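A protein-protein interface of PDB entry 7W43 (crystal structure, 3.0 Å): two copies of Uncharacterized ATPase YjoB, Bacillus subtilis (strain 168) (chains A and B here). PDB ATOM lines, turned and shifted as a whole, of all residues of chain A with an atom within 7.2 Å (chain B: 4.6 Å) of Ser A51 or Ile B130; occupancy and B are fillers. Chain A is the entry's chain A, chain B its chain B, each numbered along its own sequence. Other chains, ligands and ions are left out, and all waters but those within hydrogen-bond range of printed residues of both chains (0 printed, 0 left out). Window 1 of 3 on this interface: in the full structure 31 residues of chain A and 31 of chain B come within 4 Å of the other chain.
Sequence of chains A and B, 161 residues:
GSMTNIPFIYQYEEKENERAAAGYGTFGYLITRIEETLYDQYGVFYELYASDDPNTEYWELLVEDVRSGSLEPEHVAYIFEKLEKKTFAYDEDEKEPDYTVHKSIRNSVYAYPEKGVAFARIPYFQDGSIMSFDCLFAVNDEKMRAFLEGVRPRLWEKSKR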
ATOM      1  N   PHE A  27       9.713  -1.474  32.598  1.00  0.00           N
ATOM      2  CA  PHE A  27      10.862  -0.970  31.850  1.00  0.00           C
ATOM      3  C   PHE A  27      11.430   0.285  32.501  1.00  0.00           C
ATOM      4  O   PHE A  27      12.643   0.391  32.715  1.00  0.00           O
ATOM      5  CB  PHE A  27      10.466  -0.691  30.399  1.00  0.00           C
ATOM      6  CG  PHE A  27      11.593  -0.861  29.415  1.00  0.00           C
ATOM      7  CD1 PHE A  27      12.150  -2.107  29.182  1.00  0.00           C
ATOM      8  CD2 PHE A  27      12.098   0.230  28.729  1.00  0.00           C
ATOM      9  CE1 PHE A  27      13.187  -2.261  28.276  1.00  0.00           C
ATOM     10  CE2 PHE A  27      13.133   0.084  27.824  1.00  0.00           C
ATOM     11  CZ  PHE A  27      13.679  -1.163  27.598  1.00  0.00           C
ATOM     12  N   ILE A  31      15.110   0.161  33.892  1.00  0.00           N
ATOM     13  CA  ILE A  31      16.124   0.974  33.226  1.00  0.00           C
ATOM     14  C   ILE A  31      16.648   2.052  34.168  1.00  0.00           C
ATOM     15  O   ILE A  31      17.853   2.328  34.206  1.00  0.00           O
ATOM     16  CB  ILE A  31      15.558   1.578  31.929  1.00  0.00           C
ATOM     17  CG1 ILE A  31      15.245   0.477  30.915  1.00  0.00           C
ATOM     18  CG2 ILE A  31      16.533   2.583  31.336  1.00  0.00           C
ATOM     19  CD1 ILE A  31      16.444  -0.350  30.519  1.00  0.00           C
ATOM     20  N   LEU A  48      20.526   4.629  27.727  1.00  0.00           N
ATOM     21  CA  LEU A  48      20.120   3.592  26.789  1.00  0.00           C
ATOM     22  C   LEU A  48      20.408   4.017  25.354  1.00  0.00           C
ATOM     23  O   LEU A  48      20.090   5.138  24.948  1.00  0.00           O
ATOM     24  CB  LEU A  48      18.632   3.287  26.958  1.00  0.00           C
ATOM     25  CG  LEU A  48      18.121   1.928  26.473  1.00  0.00           C
ATOM     26  CD1 LEU A  48      18.894   0.787  27.116  1.00  0.00           C
ATOM     27  CD2 LEU A  48      16.630   1.798  26.754  1.00  0.00           C
ATOM     28  N   TYR A  49      21.015   3.113  24.585  1.00  0.00           N
ATOM     29  CA  TYR A  49      21.247   3.335  23.166  1.00  0.00           C
ATOM     30  C   TYR A  49      20.494   2.359  22.275  1.00  0.00           C
ATOM     31  O   TYR A  49      20.295   2.656  21.094  1.00  0.00           O
ATOM     32  CB  TYR A  49      22.748   3.254  22.852  1.00  0.00           C
ATOM     33  CG  TYR A  49      23.482   4.552  23.106  1.00  0.00           C
ATOM     34  CD1 TYR A  49      23.523   5.109  24.377  1.00  0.00           C
ATOM     35  CD2 TYR A  49      24.124   5.226  22.075  1.00  0.00           C
ATOM     36  CE1 TYR A  49      24.187   6.296  24.618  1.00  0.00           C
ATOM     37  CE2 TYR A  49      24.792   6.415  22.306  1.00  0.00           C
ATOM     38  CZ  TYR A  49      24.819   6.946  23.580  1.00  0.00           C
ATOM     39  OH  TYR A  49      25.482   8.129  23.815  1.00  0.00           O
ATOM     40  N   ALA A  50      20.073   1.217  22.809  1.00  0.00           N
ATOM     41  CA  ALA A  50      19.226   0.277  22.090  1.00  0.00           C
ATOM     42  C   ALA A  50      18.363  -0.443  23.114  1.00  0.00           C
ATOM     43  O   ALA A  50      18.887  -0.996  24.084  1.00  0.00           O
ATOM     44  CB  ALA A  50      20.053  -0.720  21.276  1.00  0.00           C
ATOM     45  N   SER A  51      17.044  -0.420  22.905  1.00  0.00           N
ATOM     46  CA  SER A  51      16.135  -1.005  23.886  1.00  0.00           C
ATOM     47  C   SER A  51      16.041  -2.517  23.727  1.00  0.00           C
ATOM     48  O   SER A  51      16.066  -3.252  24.721  1.00  0.00           O
ATOM     49  CB  SER A  51      14.755  -0.357  23.772  1.00  0.00           C
ATOM     50  OG  SER A  51      14.344  -0.264  22.419  1.00  0.00           O
ATOM     51  N   ASP A  52      15.929  -2.997  22.493  1.00  0.00           N
ATOM     52  CA  ASP A  52      16.025  -4.420  22.177  1.00  0.00           C
ATOM     53  C   ASP A  52      16.965  -4.535  20.983  1.00  0.00           C
ATOM     54  O   ASP A  52      16.542  -4.350  19.839  1.00  0.00           O
ATOM     55  CB  ASP A  52      14.662  -5.028  21.872  1.00  0.00           C
ATOM     56  CG  ASP A  52      14.673  -6.540  21.944  1.00  0.00           C
ATOM     57  OD1 ASP A  52      15.722  -7.108  22.319  1.00  0.00           O
ATOM     58  OD2 ASP A  52      13.637  -7.162  21.631  1.00  0.00           O
ATOM     59  N   ASP A  53      18.226  -4.841  21.255  1.00  0.00           N
ATOM     60  CA  ASP A  53      19.270  -4.810  20.238  1.00  0.00           C
ATOM     61  C   ASP A  53      19.094  -5.932  19.225  1.00  0.00           C
ATOM     62  O   ASP A  53      19.226  -7.106  19.594  1.00  0.00           O
ATOM     63  CB  ASP A  53      20.641  -4.912  20.900  1.00  0.00           C
ATOM     64  CG  ASP A  53      21.724  -4.223  20.099  1.00  0.00           C
ATOM     65  OD1 ASP A  53      21.574  -4.115  18.863  1.00  0.00           O
ATOM     66  OD2 ASP A  53      22.724  -3.791  20.706  1.00  0.00           O
ATOM     67  N   PRO A  54      18.801  -5.633  17.957  1.00  0.00           N
ATOM     68  CA  PRO A  54      18.782  -6.695  16.940  1.00  0.00           C
ATOM     69  C   PRO A  54      20.147  -7.299  16.683  1.00  0.00           C
ATOM     70  O   PRO A  54      20.221  -8.426  16.174  1.00  0.00           O
ATOM     71  CB  PRO A  54      18.257  -5.977  15.689  1.00  0.00           C
ATOM     72  CG  PRO A  54      18.568  -4.533  15.930  1.00  0.00           C
ATOM     73  CD  PRO A  54      18.398  -4.331  17.400  1.00  0.00           C
ATOM     74  N   ALA A 120      22.979  -5.093  29.138  1.00  0.00           N
ATOM     75  CA  ALA A 120      21.980  -5.658  30.034  1.00  0.00           C
ATOM     76  C   ALA A 120      21.027  -6.524  29.229  1.00  0.00           C
ATOM     77  O   ALA A 120      20.468  -6.069  28.227  1.00  0.00           O
ATOM     78  CB  ALA A 120      21.204  -4.561  30.774  1.00  0.00           C
ATOM     79  N   ILE A 122      17.746  -8.126  29.929  1.00  0.00           N
ATOM     80  CA  ILE A 122      16.652  -8.132  30.899  1.00  0.00           C
ATOM     81  C   ILE A 122      15.689  -9.275  30.604  1.00  0.00           C
ATOM     82  O   ILE A 122      15.114  -9.338  29.507  1.00  0.00           O
ATOM     83  CB  ILE A 122      15.907  -6.789  30.907  1.00  0.00           C
ATOM     84  CG1 ILE A 122      16.897  -5.627  30.952  1.00  0.00           C
ATOM     85  CG2 ILE A 122      14.950  -6.726  32.085  1.00  0.00           C
ATOM     86  CD1 ILE A 122      16.234  -4.270  31.029  1.00  0.00           C
ATOM     87  N   TYR A 124      12.154 -11.347  30.780  1.00  0.00           N
ATOM     88  CA  TYR A 124      10.747 -11.025  30.947  1.00  0.00           C
ATOM     89  C   TYR A 124       9.906 -12.253  30.642  1.00  0.00           C
ATOM     90  O   TYR A 124      10.287 -13.112  29.841  1.00  0.00           O
ATOM     91  CB  TYR A 124      10.317  -9.840  30.068  1.00  0.00           C
ATOM     92  CG  TYR A 124      10.436 -10.056  28.575  1.00  0.00           C
ATOM     93  CD1 TYR A 124       9.405 -10.647  27.858  1.00  0.00           C
ATOM     94  CD2 TYR A 124      11.563  -9.638  27.878  1.00  0.00           C
ATOM     95  CE1 TYR A 124       9.499 -10.837  26.499  1.00  0.00           C
ATOM     96  CE2 TYR A 124      11.665  -9.822  26.510  1.00  0.00           C
ATOM     97  CZ  TYR A 124      10.629 -10.420  25.826  1.00  0.00           C
ATOM     98  OH  TYR A 124      10.721 -10.611  24.466  1.00  0.00           O
ATOM     99  N   SER A 132      13.994 -12.411  26.688  1.00  0.00           N
ATOM    100  CA  SER A 132      15.006 -11.464  27.135  1.00  0.00           C
ATOM    101  C   SER A 132      15.073 -10.240  26.233  1.00  0.00           C
ATOM    102  O   SER A 132      15.028 -10.349  25.004  1.00  0.00           O
ATOM    103  CB  SER A 132      16.386 -12.126  27.200  1.00  0.00           C
ATOM    104  OG  SER A 132      16.553 -13.057  26.145  1.00  0.00           O
ATOM    105  N   PHE A 133      15.192  -9.075  26.869  1.00  0.00           N
ATOM    106  CA  PHE A 133      15.465  -7.813  26.195  1.00  0.00           C
ATOM    107  C   PHE A 133      16.968  -7.571  26.201  1.00  0.00           C
ATOM    108  O   PHE A 133      17.599  -7.620  27.260  1.00  0.00           O
ATOM    109  CB  PHE A 133      14.766  -6.658  26.915  1.00  0.00           C
ATOM    110  CG  PHE A 133      13.388  -6.351  26.410  1.00  0.00           C
ATOM    111  CD1 PHE A 133      13.142  -6.202  25.057  1.00  0.00           C
ATOM    112  CD2 PHE A 133      12.340  -6.181  27.302  1.00  0.00           C
ATOM    113  CE1 PHE A 133      11.873  -5.907  24.603  1.00  0.00           C
ATOM    114  CE2 PHE A 133      11.071  -5.886  26.853  1.00  0.00           C
ATOM    115  CZ  PHE A 133      10.840  -5.745  25.504  1.00  0.00           C
ATOM    116  N   ASP A 134      17.540  -7.296  25.034  1.00  0.00           N
ATOM    117  CA  ASP A 134      18.964  -6.976  24.927  1.00  0.00           C
ATOM    118  C   ASP A 134      19.117  -5.458  24.901  1.00  0.00           C
ATOM    119  O   ASP A 134      18.976  -4.826  23.851  1.00  0.00           O
ATOM    120  CB  ASP A 134      19.590  -7.631  23.701  1.00  0.00           C
ATOM    121  CG  ASP A 134      19.977  -9.077  23.950  1.00  0.00           C
ATOM    122  OD1 ASP A 134      19.649  -9.599  25.036  1.00  0.00           O
ATOM    123  OD2 ASP A 134      20.619  -9.688  23.069  1.00  0.00           O
ATOM    124  N   CYS A 135      19.408  -4.879  26.063  1.00  0.00           N
ATOM    125  CA  CYS A 135      19.624  -3.448  26.202  1.00  0.00           C
ATOM    126  C   CYS A 135      21.114  -3.133  26.156  1.00  0.00           C
ATOM    127  O   CYS A 135      21.949  -3.930  26.588  1.00  0.00           O
ATOM    128  CB  CYS A 135      19.030  -2.927  27.513  1.00  0.00           C
ATOM    129  SG  CYS A 135      17.274  -3.282  27.732  1.00  0.00           S
ATOM    130  N   LEU A 136      21.437  -1.954  25.631  1.00  0.00           N
ATOM    131  CA  LEU A 136      22.817  -1.508  25.500  1.00  0.00           C
ATOM    132  C   LEU A 136      22.941  -0.100  26.059  1.00  0.00           C
ATOM    133  O   LEU A 136      22.190   0.797  25.663  1.00  0.00           O
ATOM    134  CB  LEU A 136      23.276  -1.540  24.040  1.00  0.00           C
ATOM    135  CG  LEU A 136      24.790  -1.491  23.837  1.00  0.00           C
ATOM    136  CD1 LEU A 136      25.473  -2.631  24.581  1.00  0.00           C
ATOM    137  CD2 LEU A 136      25.127  -1.520  22.359  1.00  0.00           C
ATOM    138  N   GLU B  84      15.027   4.466  24.503  1.00  0.00           N
ATOM    139  CA  GLU B  84      16.205   4.917  23.773  1.00  0.00           C
ATOM    140  C   GLU B  84      16.114   6.405  23.468  1.00  0.00           C
ATOM    141  O   GLU B  84      15.103   6.886  22.949  1.00  0.00           O
ATOM    142  CB  GLU B  84      16.363   4.138  22.466  1.00  0.00           C
ATOM    143  CG  GLU B  84      15.057   3.751  21.804  1.00  0.00           C
ATOM    144  CD  GLU B  84      15.272   2.952  20.536  1.00  0.00           C
ATOM    145  OE1 GLU B  84      15.882   1.865  20.607  1.00  0.00           O
ATOM    146  OE2 GLU B  84      14.840   3.423  19.462  1.00  0.00           O
ATOM    147  N   ARG B 106      12.969   6.165  16.645  1.00  0.00           N
ATOM    148  CA  ARG B 106      11.962   5.640  17.553  1.00  0.00           C
ATOM    149  C   ARG B 106      12.078   6.345  18.899  1.00  0.00           C
ATOM    150  O   ARG B 106      13.183   6.626  19.368  1.00  0.00           O
ATOM    151  CB  ARG B 106      12.134   4.130  17.719  1.00  0.00           C
ATOM    152  CG  ARG B 106      11.019   3.443  18.485  1.00  0.00           C
ATOM    153  CD  ARG B 106      11.132   1.928  18.379  1.00  0.00           C
ATOM    154  NE  ARG B 106      12.188   1.391  19.233  1.00  0.00           N
ATOM    155  CZ  ARG B 106      12.611   0.131  19.201  1.00  0.00           C
ATOM    156  NH1 ARG B 106      12.063  -0.735  18.358  1.00  0.00           N
ATOM    157  NH2 ARG B 106      13.578  -0.266  20.017  1.00  0.00           N
ATOM    158  N   PRO B 123       6.587   4.191  20.467  1.00  0.00           N
ATOM    159  CA  PRO B 123       6.871   2.799  20.821  1.00  0.00           C
ATOM    160  C   PRO B 123       5.788   2.180  21.696  1.00  0.00           C
ATOM    161  O   PRO B 123       5.031   2.866  22.385  1.00  0.00           O
ATOM    162  CB  PRO B 123       8.200   2.908  21.593  1.00  0.00           C
ATOM    163  CG  PRO B 123       8.617   4.396  21.465  1.00  0.00           C
ATOM    164  CD  PRO B 123       7.313   5.099  21.361  1.00  0.00           C
ATOM    165  N   TYR B 124       5.732   0.848  21.654  1.00  0.00           N
ATOM    166  CA  TYR B 124       4.776   0.097  22.454  1.00  0.00           C
ATOM    167  C   TYR B 124       5.288  -1.322  22.659  1.00  0.00           C
ATOM    168  O   TYR B 124       6.159  -1.804  21.929  1.00  0.00           O
ATOM    169  CB  TYR B 124       3.381   0.084  21.811  1.00  0.00           C
ATOM    170  CG  TYR B 124       3.312  -0.563  20.443  1.00  0.00           C
ATOM    171  CD1 TYR B 124       3.616   0.156  19.293  1.00  0.00           C
ATOM    172  CD2 TYR B 124       2.942  -1.893  20.302  1.00  0.00           C
ATOM    173  CE1 TYR B 124       3.548  -0.432  18.042  1.00  0.00           C
ATOM    174  CE2 TYR B 124       2.875  -2.488  19.060  1.00  0.00           C
ATOM    175  CZ  TYR B 124       3.174  -1.754  17.932  1.00  0.00           C
ATOM    176  OH  TYR B 124       3.109  -2.352  16.694  1.00  0.00           O
ATOM    177  N   PHE B 125       4.735  -1.986  23.672  1.00  0.00           N
ATOM    178  CA  PHE B 125       5.131  -3.334  24.062  1.00  0.00           C
ATOM    179  C   PHE B 125       4.026  -4.308  23.672  1.00  0.00           C
ATOM    180  O   PHE B 125       2.881  -4.162  24.115  1.00  0.00           O
ATOM    181  CB  PHE B 125       5.401  -3.411  25.567  1.00  0.00           C
ATOM    182  CG  PHE B 125       6.623  -2.648  26.016  1.00  0.00           C
ATOM    183  CD1 PHE B 125       6.541  -1.303  26.341  1.00  0.00           C
ATOM    184  CD2 PHE B 125       7.849  -3.285  26.136  1.00  0.00           C
ATOM    185  CE1 PHE B 125       7.662  -0.604  26.763  1.00  0.00           C
ATOM    186  CE2 PHE B 125       8.972  -2.592  26.558  1.00  0.00           C
ATOM    187  CZ  PHE B 125       8.877  -1.249  26.871  1.00  0.00           C
ATOM    188  N   GLY B 128       6.087  -9.267  24.047  1.00  0.00           N
ATOM    189  CA  GLY B 128       7.507  -9.226  24.319  1.00  0.00           C
ATOM    190  C   GLY B 128       8.223  -8.078  23.646  1.00  0.00           C
ATOM    191  O   GLY B 128       8.561  -7.088  24.298  1.00  0.00           O
ATOM    192  N   SER B 129       8.438  -8.189  22.339  1.00  0.00           N
ATOM    193  CA  SER B 129       9.271  -7.242  21.614  1.00  0.00           C
ATOM    194  C   SER B 129       8.671  -5.838  21.634  1.00  0.00           C
ATOM    195  O   SER B 129       7.464  -5.644  21.804  1.00  0.00           O
ATOM    196  CB  SER B 129       9.463  -7.704  20.171  1.00  0.00           C
ATOM    197  OG  SER B 129       9.932  -9.041  20.125  1.00  0.00           O
ATOM    198  N   ILE B 130       9.546  -4.851  21.460  1.00  0.00           N
ATOM    199  CA  ILE B 130       9.148  -3.452  21.350  1.00  0.00           C
ATOM    200  C   ILE B 130       8.936  -3.124  19.879  1.00  0.00           C
ATOM    201  O   ILE B 130       9.803  -3.397  19.039  1.00  0.00           O
ATOM    202  CB  ILE B 130      10.206  -2.525  21.971  1.00  0.00           C
ATOM    203  CG1 ILE B 130      10.499  -2.930  23.416  1.00  0.00           C
ATOM    204  CG2 ILE B 130       9.750  -1.078  21.912  1.00  0.00           C
ATOM    205  CD1 ILE B 130      11.529  -2.057  24.097  1.00  0.00           C
ATOM    206  N   MET B 131       7.784  -2.545  19.564  1.00  0.00           N
ATOM    207  CA  MET B 131       7.441  -2.135  18.210  1.00  0.00           C
ATOM    208  C   MET B 131       7.202  -0.625  18.201  1.00  0.00           C
ATOM    209  O   MET B 131       7.442   0.066  19.195  1.00  0.00           O
ATOM    210  CB  MET B 131       6.231  -2.926  17.709  1.00  0.00           C
ATOM    211  CG  MET B 131       6.114  -4.310  18.328  1.00  0.00           C
ATOM    212  SD  MET B 131       4.624  -5.200  17.843  1.00  0.00           S
ATOM    213  CE  MET B 131       5.084  -5.740  16.202  1.00  0.00           C
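The side-chain hydroxyl of Ser A51 lies within hydrogen-bond range of the side-chain carboxylate of Glu B84, at 3.2 Å.
OG of Ser A51 lies within hydrogen-bond range of NH2 of Arg B106 (2.5 Å).
1 position is printed for both chains.
Ser A51 touches three residues of chain B.
Ile B130 touches just these residues of chain A: Ser A51 and Phe A133.
Printed residues of chain A within 4 Å of Arg B106: Ser A51 (2.5 Å).
Printed residues of chain B within 4 Å of Ala A50: Glu B84 (3.99 Å).
Tyr B124 touches none of the printed residues of chain A.
Asp A53 touches none of the printed residues of chain B.
Of the 17 printed residues of chain A, 6 touch a printed residue of chain B.
Hydrophobic or aromatic side chains of chain A within 4 Å of the printed part of chain B: Phe A27, Leu A48, Tyr A124 and Phe A133.
Along chain A the printed residues that touch a printed residue of chain B span positions 27 to 133.
CG of Phe A27 touches CZ of Phe B125, 3.7 Å away.
CD2 of Leu A48 touches N of Glu B84, at 3.8 Å.
OE1 of Glu B84 touches CA of Ala A50, 3.99 Å away.
CB of Ser A51 touches CD1 of Ile B130 (3.7 Å).
Tyr A124 touches Gly B128.
Ser B129 touches Tyr A124 (N to OH, 3.9 Å).
Phe A133 touches Phe B125.
Phe A133 touches Gly B128.
Phe A133 touches Ile B130.
The backbone carbonyl oxygen (O) of Ala A50 is in hydrogen-bond range of the backbone NH (N) of Leu A136, 3.1 Å away.
OE1 of Glu B84 lies within salt-bridge range of NH2 of Arg B106, at 3.2 Å.
The backbone NH (N) of Phe A133 is in hydrogen-bond range of the backbone carbonyl oxygen (O) of Ile A122, 2.7 Å away.
The backbone carbonyl oxygen of Ser A51 is in hydrogen-bond range of the side-chain sulfur of Cys A135, at 3.2 Å.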
